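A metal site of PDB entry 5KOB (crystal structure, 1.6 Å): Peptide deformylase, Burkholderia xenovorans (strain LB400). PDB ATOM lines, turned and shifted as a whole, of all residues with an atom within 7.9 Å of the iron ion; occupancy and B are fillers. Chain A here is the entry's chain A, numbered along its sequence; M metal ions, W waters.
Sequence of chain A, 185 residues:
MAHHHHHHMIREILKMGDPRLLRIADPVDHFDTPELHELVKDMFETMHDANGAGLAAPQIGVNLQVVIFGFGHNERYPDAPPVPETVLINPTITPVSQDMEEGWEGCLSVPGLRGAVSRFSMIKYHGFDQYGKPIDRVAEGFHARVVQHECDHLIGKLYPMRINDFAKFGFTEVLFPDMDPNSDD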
ATOM      1  N   ILE A  13       3.132 -13.349 -33.324  1.00  0.00           N
ATOM      2  CA  ILE A  13       3.212 -12.575 -32.088  1.00  0.00           C
ATOM      3  C   ILE A  13       4.363 -13.109 -31.253  1.00  0.00           C
ATOM      4  O   ILE A  13       4.421 -14.310 -30.955  1.00  0.00           O
ATOM      5  CB  ILE A  13       1.886 -12.653 -31.312  1.00  0.00           C
ATOM      6  CG1 ILE A  13       0.737 -12.133 -32.174  1.00  0.00           C
ATOM      7  CG2 ILE A  13       1.986 -11.890 -29.976  1.00  0.00           C
ATOM      8  CD1 ILE A  13      -0.634 -12.337 -31.588  1.00  0.00           C
ATOM      9  N   LEU A  21      10.552  -7.471 -26.797  1.00  0.00           N
ATOM     10  CA  LEU A  21       9.456  -6.965 -25.989  1.00  0.00           C
ATOM     11  C   LEU A  21       9.933  -6.087 -24.834  1.00  0.00           C
ATOM     12  O   LEU A  21       9.093  -5.650 -24.033  1.00  0.00           O
ATOM     13  CB  LEU A  21       8.642  -8.146 -25.423  1.00  0.00           C
ATOM     14  CG  LEU A  21       7.985  -9.014 -26.504  1.00  0.00           C
ATOM     15  CD1 LEU A  21       7.396 -10.278 -25.849  1.00  0.00           C
ATOM     16  CD2 LEU A  21       6.915  -8.225 -27.268  1.00  0.00           C
ATOM     17  N   GLY A  54      -6.061  -5.540 -28.036  1.00  0.00           N
ATOM     18  CA  GLY A  54      -5.138  -4.527 -28.533  1.00  0.00           C
ATOM     19  C   GLY A  54      -3.876  -5.215 -28.998  1.00  0.00           C
ATOM     20  O   GLY A  54      -3.683  -6.405 -28.779  1.00  0.00           O
ATOM     21  N   LEU A  55      -3.017  -4.440 -29.653  1.00  0.00           N
ATOM     22  CA  LEU A  55      -1.731  -4.973 -30.099  1.00  0.00           C
ATOM     23  C   LEU A  55      -0.790  -3.799 -30.291  1.00  0.00           C
ATOM     24  O   LEU A  55      -1.211  -2.728 -30.738  1.00  0.00           O
ATOM     25  CB  LEU A  55      -1.869  -5.743 -31.416  1.00  0.00           C
ATOM     26  CG  LEU A  55      -0.665  -6.615 -31.788  1.00  0.00           C
ATOM     27  CD1 LEU A  55      -0.626  -7.899 -30.965  1.00  0.00           C
ATOM     28  CD2 LEU A  55      -0.672  -6.922 -33.298  1.00  0.00           C
ATOM     29  N   ALA A  56       0.486  -4.014 -29.966  1.00  0.00           N
ATOM     30  CA  ALA A  56       1.521  -2.998 -30.144  1.00  0.00           C
ATOM     31  C   ALA A  56       2.561  -3.508 -31.124  1.00  0.00           C
ATOM     32  O   ALA A  56       2.847  -4.709 -31.158  1.00  0.00           O
ATOM     33  CB  ALA A  56       2.172  -2.638 -28.797  1.00  0.00           C
ATOM     34  N   GLN A  59       5.191  -6.194 -30.495  1.00  0.00           N
ATOM     35  CA  GLN A  59       4.748  -7.578 -30.382  1.00  0.00           C
ATOM     36  C   GLN A  59       4.864  -8.360 -31.676  1.00  0.00           C
ATOM     37  O   GLN A  59       4.798  -9.593 -31.644  1.00  0.00           O
ATOM     38  CB  GLN A  59       3.293  -7.642 -29.890  1.00  0.00           C
ATOM     39  CG  GLN A  59       3.113  -7.159 -28.448  1.00  0.00           C
ATOM     40  CD  GLN A  59       1.655  -7.304 -28.019  1.00  0.00           C
ATOM     41  OE1 GLN A  59       0.864  -6.384 -28.218  1.00  0.00           O
ATOM     42  NE2 GLN A  59       1.297  -8.468 -27.462  1.00  0.00           N
ATOM     43  N   TYR A  77     -12.234 -11.230 -23.137  1.00  0.00           N
ATOM     44  CA  TYR A  77     -12.629 -10.282 -22.104  1.00  0.00           C
ATOM     45  C   TYR A  77     -14.138 -10.060 -22.206  1.00  0.00           C
ATOM     46  O   TYR A  77     -14.607  -8.956 -22.512  1.00  0.00           O
ATOM     47  CB  TYR A  77     -11.866  -8.969 -22.218  1.00  0.00           C
ATOM     48  CG  TYR A  77     -10.373  -9.149 -22.127  1.00  0.00           C
ATOM     49  CD1 TYR A  77      -9.744  -9.211 -20.884  1.00  0.00           C
ATOM     50  CD2 TYR A  77      -9.593  -9.254 -23.265  1.00  0.00           C
ATOM     51  CE1 TYR A  77      -8.359  -9.381 -20.798  1.00  0.00           C
ATOM     52  CE2 TYR A  77      -8.224  -9.424 -23.195  1.00  0.00           C
ATOM     53  CZ  TYR A  77      -7.616  -9.494 -21.949  1.00  0.00           C
ATOM     54  OH  TYR A  77      -6.250  -9.655 -21.876  1.00  0.00           O
ATOM     55  N   GLU A 105      -5.794  -8.557 -16.249  1.00  0.00           N
ATOM     56  CA  GLU A 105      -5.242  -8.346 -17.579  1.00  0.00           C
ATOM     57  C   GLU A 105      -4.606  -9.612 -18.121  1.00  0.00           C
ATOM     58  O   GLU A 105      -4.027 -10.410 -17.377  1.00  0.00           O
ATOM     59  CB  GLU A 105      -4.189  -7.241 -17.589  1.00  0.00           C
ATOM     60  CG  GLU A 105      -4.770  -5.888 -17.220  1.00  0.00           C
ATOM     61  CD  GLU A 105      -3.836  -4.737 -17.499  1.00  0.00           C
ATOM     62  OE1 GLU A 105      -2.857  -4.909 -18.276  1.00  0.00           O
ATOM     63  OE2 GLU A 105      -4.068  -3.663 -16.935  1.00  0.00           O
ATOM     64  N   GLY A 106      -4.716  -9.766 -19.439  1.00  0.00           N
ATOM     65  CA  GLY A 106      -3.951 -10.739 -20.190  1.00  0.00           C
ATOM     66  C   GLY A 106      -3.180 -10.023 -21.288  1.00  0.00           C
ATOM     67  O   GLY A 106      -3.229  -8.803 -21.412  1.00  0.00           O
ATOM     68  N   CYS A 107      -2.493 -10.831 -22.101  1.00  0.00           N
ATOM     69  CA  CYS A 107      -1.636 -10.283 -23.158  1.00  0.00           C
ATOM     70  C   CYS A 107      -1.396 -11.382 -24.179  1.00  0.00           C
ATOM     71  O   CYS A 107      -1.117 -12.522 -23.808  1.00  0.00           O
ATOM     72  CB  CYS A 107      -0.299  -9.786 -22.591  1.00  0.00           C
ATOM     73  SG  CYS A 107       0.785  -8.989 -23.824  1.00  0.00           S
ATOM     74  N   LEU A 108      -1.470 -11.043 -25.474  1.00  0.00           N
ATOM     75  CA  LEU A 108      -1.207 -12.047 -26.499  1.00  0.00           C
ATOM     76  C   LEU A 108       0.254 -12.512 -26.475  1.00  0.00           C
ATOM     77  O   LEU A 108       0.553 -13.604 -26.972  1.00  0.00           O
ATOM     78  CB  LEU A 108      -1.585 -11.521 -27.878  1.00  0.00           C
ATOM     79  CG  LEU A 108      -3.076 -11.271 -28.108  1.00  0.00           C
ATOM     80  CD1 LEU A 108      -3.310 -10.685 -29.502  1.00  0.00           C
ATOM     81  CD2 LEU A 108      -3.870 -12.574 -27.944  1.00  0.00           C
ATOM     82  N   SER A 109       1.140 -11.716 -25.895  1.00  0.00           N
ATOM     83  CA  SER A 109       2.522 -12.143 -25.705  1.00  0.00           C
ATOM     84  C   SER A 109       2.708 -12.961 -24.430  1.00  0.00           C
ATOM     85  O   SER A 109       3.806 -13.471 -24.184  1.00  0.00           O
ATOM     86  CB  SER A 109       3.468 -10.934 -25.662  1.00  0.00           C
ATOM     87  OG  SER A 109       3.575 -10.303 -26.944  1.00  0.00           O
ATOM     88  N   VAL A 110       1.659 -13.111 -23.624  1.00  0.00           N
ATOM     89  CA  VAL A 110       1.740 -13.917 -22.397  1.00  0.00           C
ATOM     90  C   VAL A 110       0.589 -14.915 -22.420  1.00  0.00           C
ATOM     91  O   VAL A 110      -0.297 -14.905 -21.533  1.00  0.00           O
ATOM     92  CB  VAL A 110       1.700 -13.025 -21.140  1.00  0.00           C
ATOM     93  CG1 VAL A 110       2.075 -13.849 -19.903  1.00  0.00           C
ATOM     94  CG2 VAL A 110       2.652 -11.827 -21.288  1.00  0.00           C
ATOM     95  N   ARG A 119      -4.399   0.240 -12.817  1.00  0.00           N
ATOM     96  CA  ARG A 119      -4.256   1.235 -13.881  1.00  0.00           C
ATOM     97  C   ARG A 119      -4.988   2.504 -13.464  1.00  0.00           C
ATOM     98  O   ARG A 119      -5.891   2.466 -12.621  1.00  0.00           O
ATOM     99  CB  ARG A 119      -4.843   0.761 -15.217  1.00  0.00           C
ATOM    100  CG  ARG A 119      -4.237  -0.527 -15.753  1.00  0.00           C
ATOM    101  CD  ARG A 119      -2.822  -0.323 -16.249  1.00  0.00           C
ATOM    102  NE  ARG A 119      -2.342  -1.534 -16.936  1.00  0.00           N
ATOM    103  CZ  ARG A 119      -1.115  -1.663 -17.462  1.00  0.00           C
ATOM    104  NH1 ARG A 119      -0.245  -0.661 -17.384  1.00  0.00           N
ATOM    105  NH2 ARG A 119      -0.770  -2.813 -18.054  1.00  0.00           N
ATOM    106  N   VAL A 146      -6.828  -0.606 -21.558  1.00  0.00           N
ATOM    107  CA  VAL A 146      -6.217  -1.118 -22.791  1.00  0.00           C
ATOM    108  C   VAL A 146      -5.181  -0.127 -23.319  1.00  0.00           C
ATOM    109  O   VAL A 146      -4.104  -0.515 -23.783  1.00  0.00           O
ATOM    110  CB  VAL A 146      -7.295  -1.401 -23.845  1.00  0.00           C
ATOM    111  CG1 VAL A 146      -6.668  -1.665 -25.215  1.00  0.00           C
ATOM    112  CG2 VAL A 146      -8.145  -2.577 -23.420  1.00  0.00           C
ATOM    113  N   HIS A 149      -2.085  -0.400 -21.172  1.00  0.00           N
ATOM    114  CA  HIS A 149      -1.418  -1.678 -21.434  1.00  0.00           C
ATOM    115  C   HIS A 149      -0.634  -1.629 -22.735  1.00  0.00           C
ATOM    116  O   HIS A 149       0.517  -2.057 -22.808  1.00  0.00           O
ATOM    117  CB  HIS A 149      -2.466  -2.781 -21.467  1.00  0.00           C
ATOM    118  CG  HIS A 149      -1.917  -4.142 -21.803  1.00  0.00           C
ATOM    119  ND1 HIS A 149      -1.904  -5.167 -20.883  1.00  0.00           N
ATOM    120  CD2 HIS A 149      -1.414  -4.645 -22.954  1.00  0.00           C
ATOM    121  CE1 HIS A 149      -1.382  -6.238 -21.441  1.00  0.00           C
ATOM    122  NE2 HIS A 149      -1.089  -5.955 -22.697  1.00  0.00           N
ATOM    123  N   GLU A 150      -1.253  -1.071 -23.797  1.00  0.00           N
ATOM    124  CA  GLU A 150      -0.580  -1.070 -25.092  1.00  0.00           C
ATOM    125  C   GLU A 150       0.578  -0.080 -25.113  1.00  0.00           C
ATOM    126  O   GLU A 150       1.645  -0.397 -25.653  1.00  0.00           O
ATOM    127  CB  GLU A 150      -1.584  -0.750 -26.204  1.00  0.00           C
ATOM    128  CG  GLU A 150      -2.630  -1.826 -26.414  1.00  0.00           C
ATOM    129  CD  GLU A 150      -2.048  -3.210 -26.584  1.00  0.00           C
ATOM    130  OE1 GLU A 150      -0.937  -3.328 -27.128  1.00  0.00           O
ATOM    131  OE2 GLU A 150      -2.698  -4.188 -26.174  1.00  0.00           O
ATOM    132  N   ASP A 152       2.373   0.685 -22.639  1.00  0.00           N
ATOM    133  CA  ASP A 152       3.449   0.058 -21.869  1.00  0.00           C
ATOM    134  C   ASP A 152       4.376  -0.758 -22.772  1.00  0.00           C
ATOM    135  O   ASP A 152       5.592  -0.805 -22.534  1.00  0.00           O
ATOM    136  CB  ASP A 152       2.881  -0.843 -20.770  1.00  0.00           C
ATOM    137  CG  ASP A 152       2.935  -0.223 -19.399  1.00  0.00           C
ATOM    138  OD1 ASP A 152       3.374   0.936 -19.243  1.00  0.00           O
ATOM    139  OD2 ASP A 152       2.526  -0.928 -18.438  1.00  0.00           O
ATOM    140  N   HIS A 153       3.813  -1.470 -23.758  1.00  0.00           N
ATOM    141  CA  HIS A 153       4.648  -2.234 -24.679  1.00  0.00           C
ATOM    142  C   HIS A 153       5.703  -1.365 -25.333  1.00  0.00           C
ATOM    143  O   HIS A 153       6.800  -1.855 -25.641  1.00  0.00           O
ATOM    144  CB  HIS A 153       3.800  -2.870 -25.762  1.00  0.00           C
ATOM    145  CG  HIS A 153       3.149  -4.138 -25.325  1.00  0.00           C
ATOM    146  ND1 HIS A 153       3.865  -5.229 -24.901  1.00  0.00           N
ATOM    147  CD2 HIS A 153       1.842  -4.488 -25.280  1.00  0.00           C
ATOM    148  CE1 HIS A 153       3.029  -6.214 -24.601  1.00  0.00           C
ATOM    149  NE2 HIS A 153       1.800  -5.784 -24.825  1.00  0.00           N
ATOM    150  N   LYS A 157       7.556  -2.705 -21.348  1.00  0.00           N
ATOM    151  CA  LYS A 157       6.899  -3.188 -20.134  1.00  0.00           C
ATOM    152  C   LYS A 157       5.794  -4.175 -20.504  1.00  0.00           C
ATOM    153  O   LYS A 157       4.928  -3.855 -21.336  1.00  0.00           O
ATOM    154  CB  LYS A 157       6.320  -2.032 -19.320  1.00  0.00           C
ATOM    155  CG  LYS A 157       7.304  -0.993 -18.888  1.00  0.00           C
ATOM    156  CD  LYS A 157       8.234  -1.527 -17.829  1.00  0.00           C
ATOM    157  CE  LYS A 157       8.941  -0.380 -17.118  1.00  0.00           C
ATOM    158  NZ  LYS A 157      10.155  -0.849 -16.407  1.00  0.00           N
ATOM    159  N   LEU A 158       5.838  -5.348 -19.881  1.00  0.00           N
ATOM    160  CA  LEU A 158       4.831  -6.376 -19.985  1.00  0.00           C
ATOM    161  C   LEU A 158       4.091  -6.389 -18.647  1.00  0.00           C
ATOM    162  O   LEU A 158       4.675  -6.051 -17.613  1.00  0.00           O
ATOM    163  CB  LEU A 158       5.449  -7.739 -20.270  1.00  0.00           C
ATOM    164  CG  LEU A 158       6.365  -7.751 -21.512  1.00  0.00           C
ATOM    165  CD1 LEU A 158       7.098  -9.082 -21.621  1.00  0.00           C
ATOM    166  CD2 LEU A 158       5.534  -7.499 -22.732  1.00  0.00           C
ATOM    167  N   TYR A 159       2.818  -6.770 -18.648  1.00  0.00           N
ATOM    168  CA  TYR A 159       2.039  -6.557 -17.427  1.00  0.00           C
ATOM    169  C   TYR A 159       2.561  -7.300 -16.195  1.00  0.00           C
ATOM    170  O   TYR A 159       2.339  -6.772 -15.089  1.00  0.00           O
ATOM    171  CB  TYR A 159       0.546  -6.862 -17.648  1.00  0.00           C
ATOM    172  CG  TYR A 159       0.174  -8.299 -17.699  1.00  0.00           C
ATOM    173  CD1 TYR A 159      -0.121  -8.995 -16.516  1.00  0.00           C
ATOM    174  CD2 TYR A 159       0.084  -8.988 -18.897  1.00  0.00           C
ATOM    175  CE1 TYR A 159      -0.462 -10.321 -16.540  1.00  0.00           C
ATOM    176  CE2 TYR A 159      -0.270 -10.336 -18.933  1.00  0.00           C
ATOM    177  CZ  TYR A 159      -0.544 -10.996 -17.741  1.00  0.00           C
ATOM    178  OH  TYR A 159      -0.877 -12.337 -17.780  1.00  0.00           O
HETATM  179 FE    FE M   1      -0.043  -6.881 -24.375  1.00  0.00          FE
HETATM  180  O   HOH W   1      -1.215  -6.183 -26.157  1.00  0.00           O
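A ring nitrogen (ND1) of His 149 is in hydrogen-bond range of the side-chain carboxylate (OE1) of Glu 105 (2.8 Å). SG of Cys 107 sits close to NE2 of Gln 59, 3.7 Å away. The side-chain sulfur of Cys 107 lies close to the backbone NH of Ser 109 (3.4 Å). The side-chain amide nitrogen (NE2) of Gln 59 lies within hydrogen-bond range of the side-chain hydroxyl (OG) of Ser 109 (3.0 Å). OE1 of Gln 59 is in hydrogen-bond range of N of Ala 56 (3.0 Å).
Residues that only touch the iron ion: Gln 59 (3.7 Å). Of the 22 residues printed, 4 come within 4 Å of the iron ion. The nearest printed residue that does not touch the iron ion is Glu 150 (4.2 Å).
The iron ion is bound by a ring nitrogen (NE2) of His 149, at 2.2 Å. A ring nitrogen (NE2) of His 153 binds the iron ion (2.2 Å). The iron ion is bound by water W1, 2.2 Å away. SG of Cys 107 binds the iron ion.
Water W1 lies within hydrogen-bond range of the side-chain carboxylate of Glu 150 (2.5 Å) and the side-chain amide oxygen of Gln 59 (2.9 Å).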
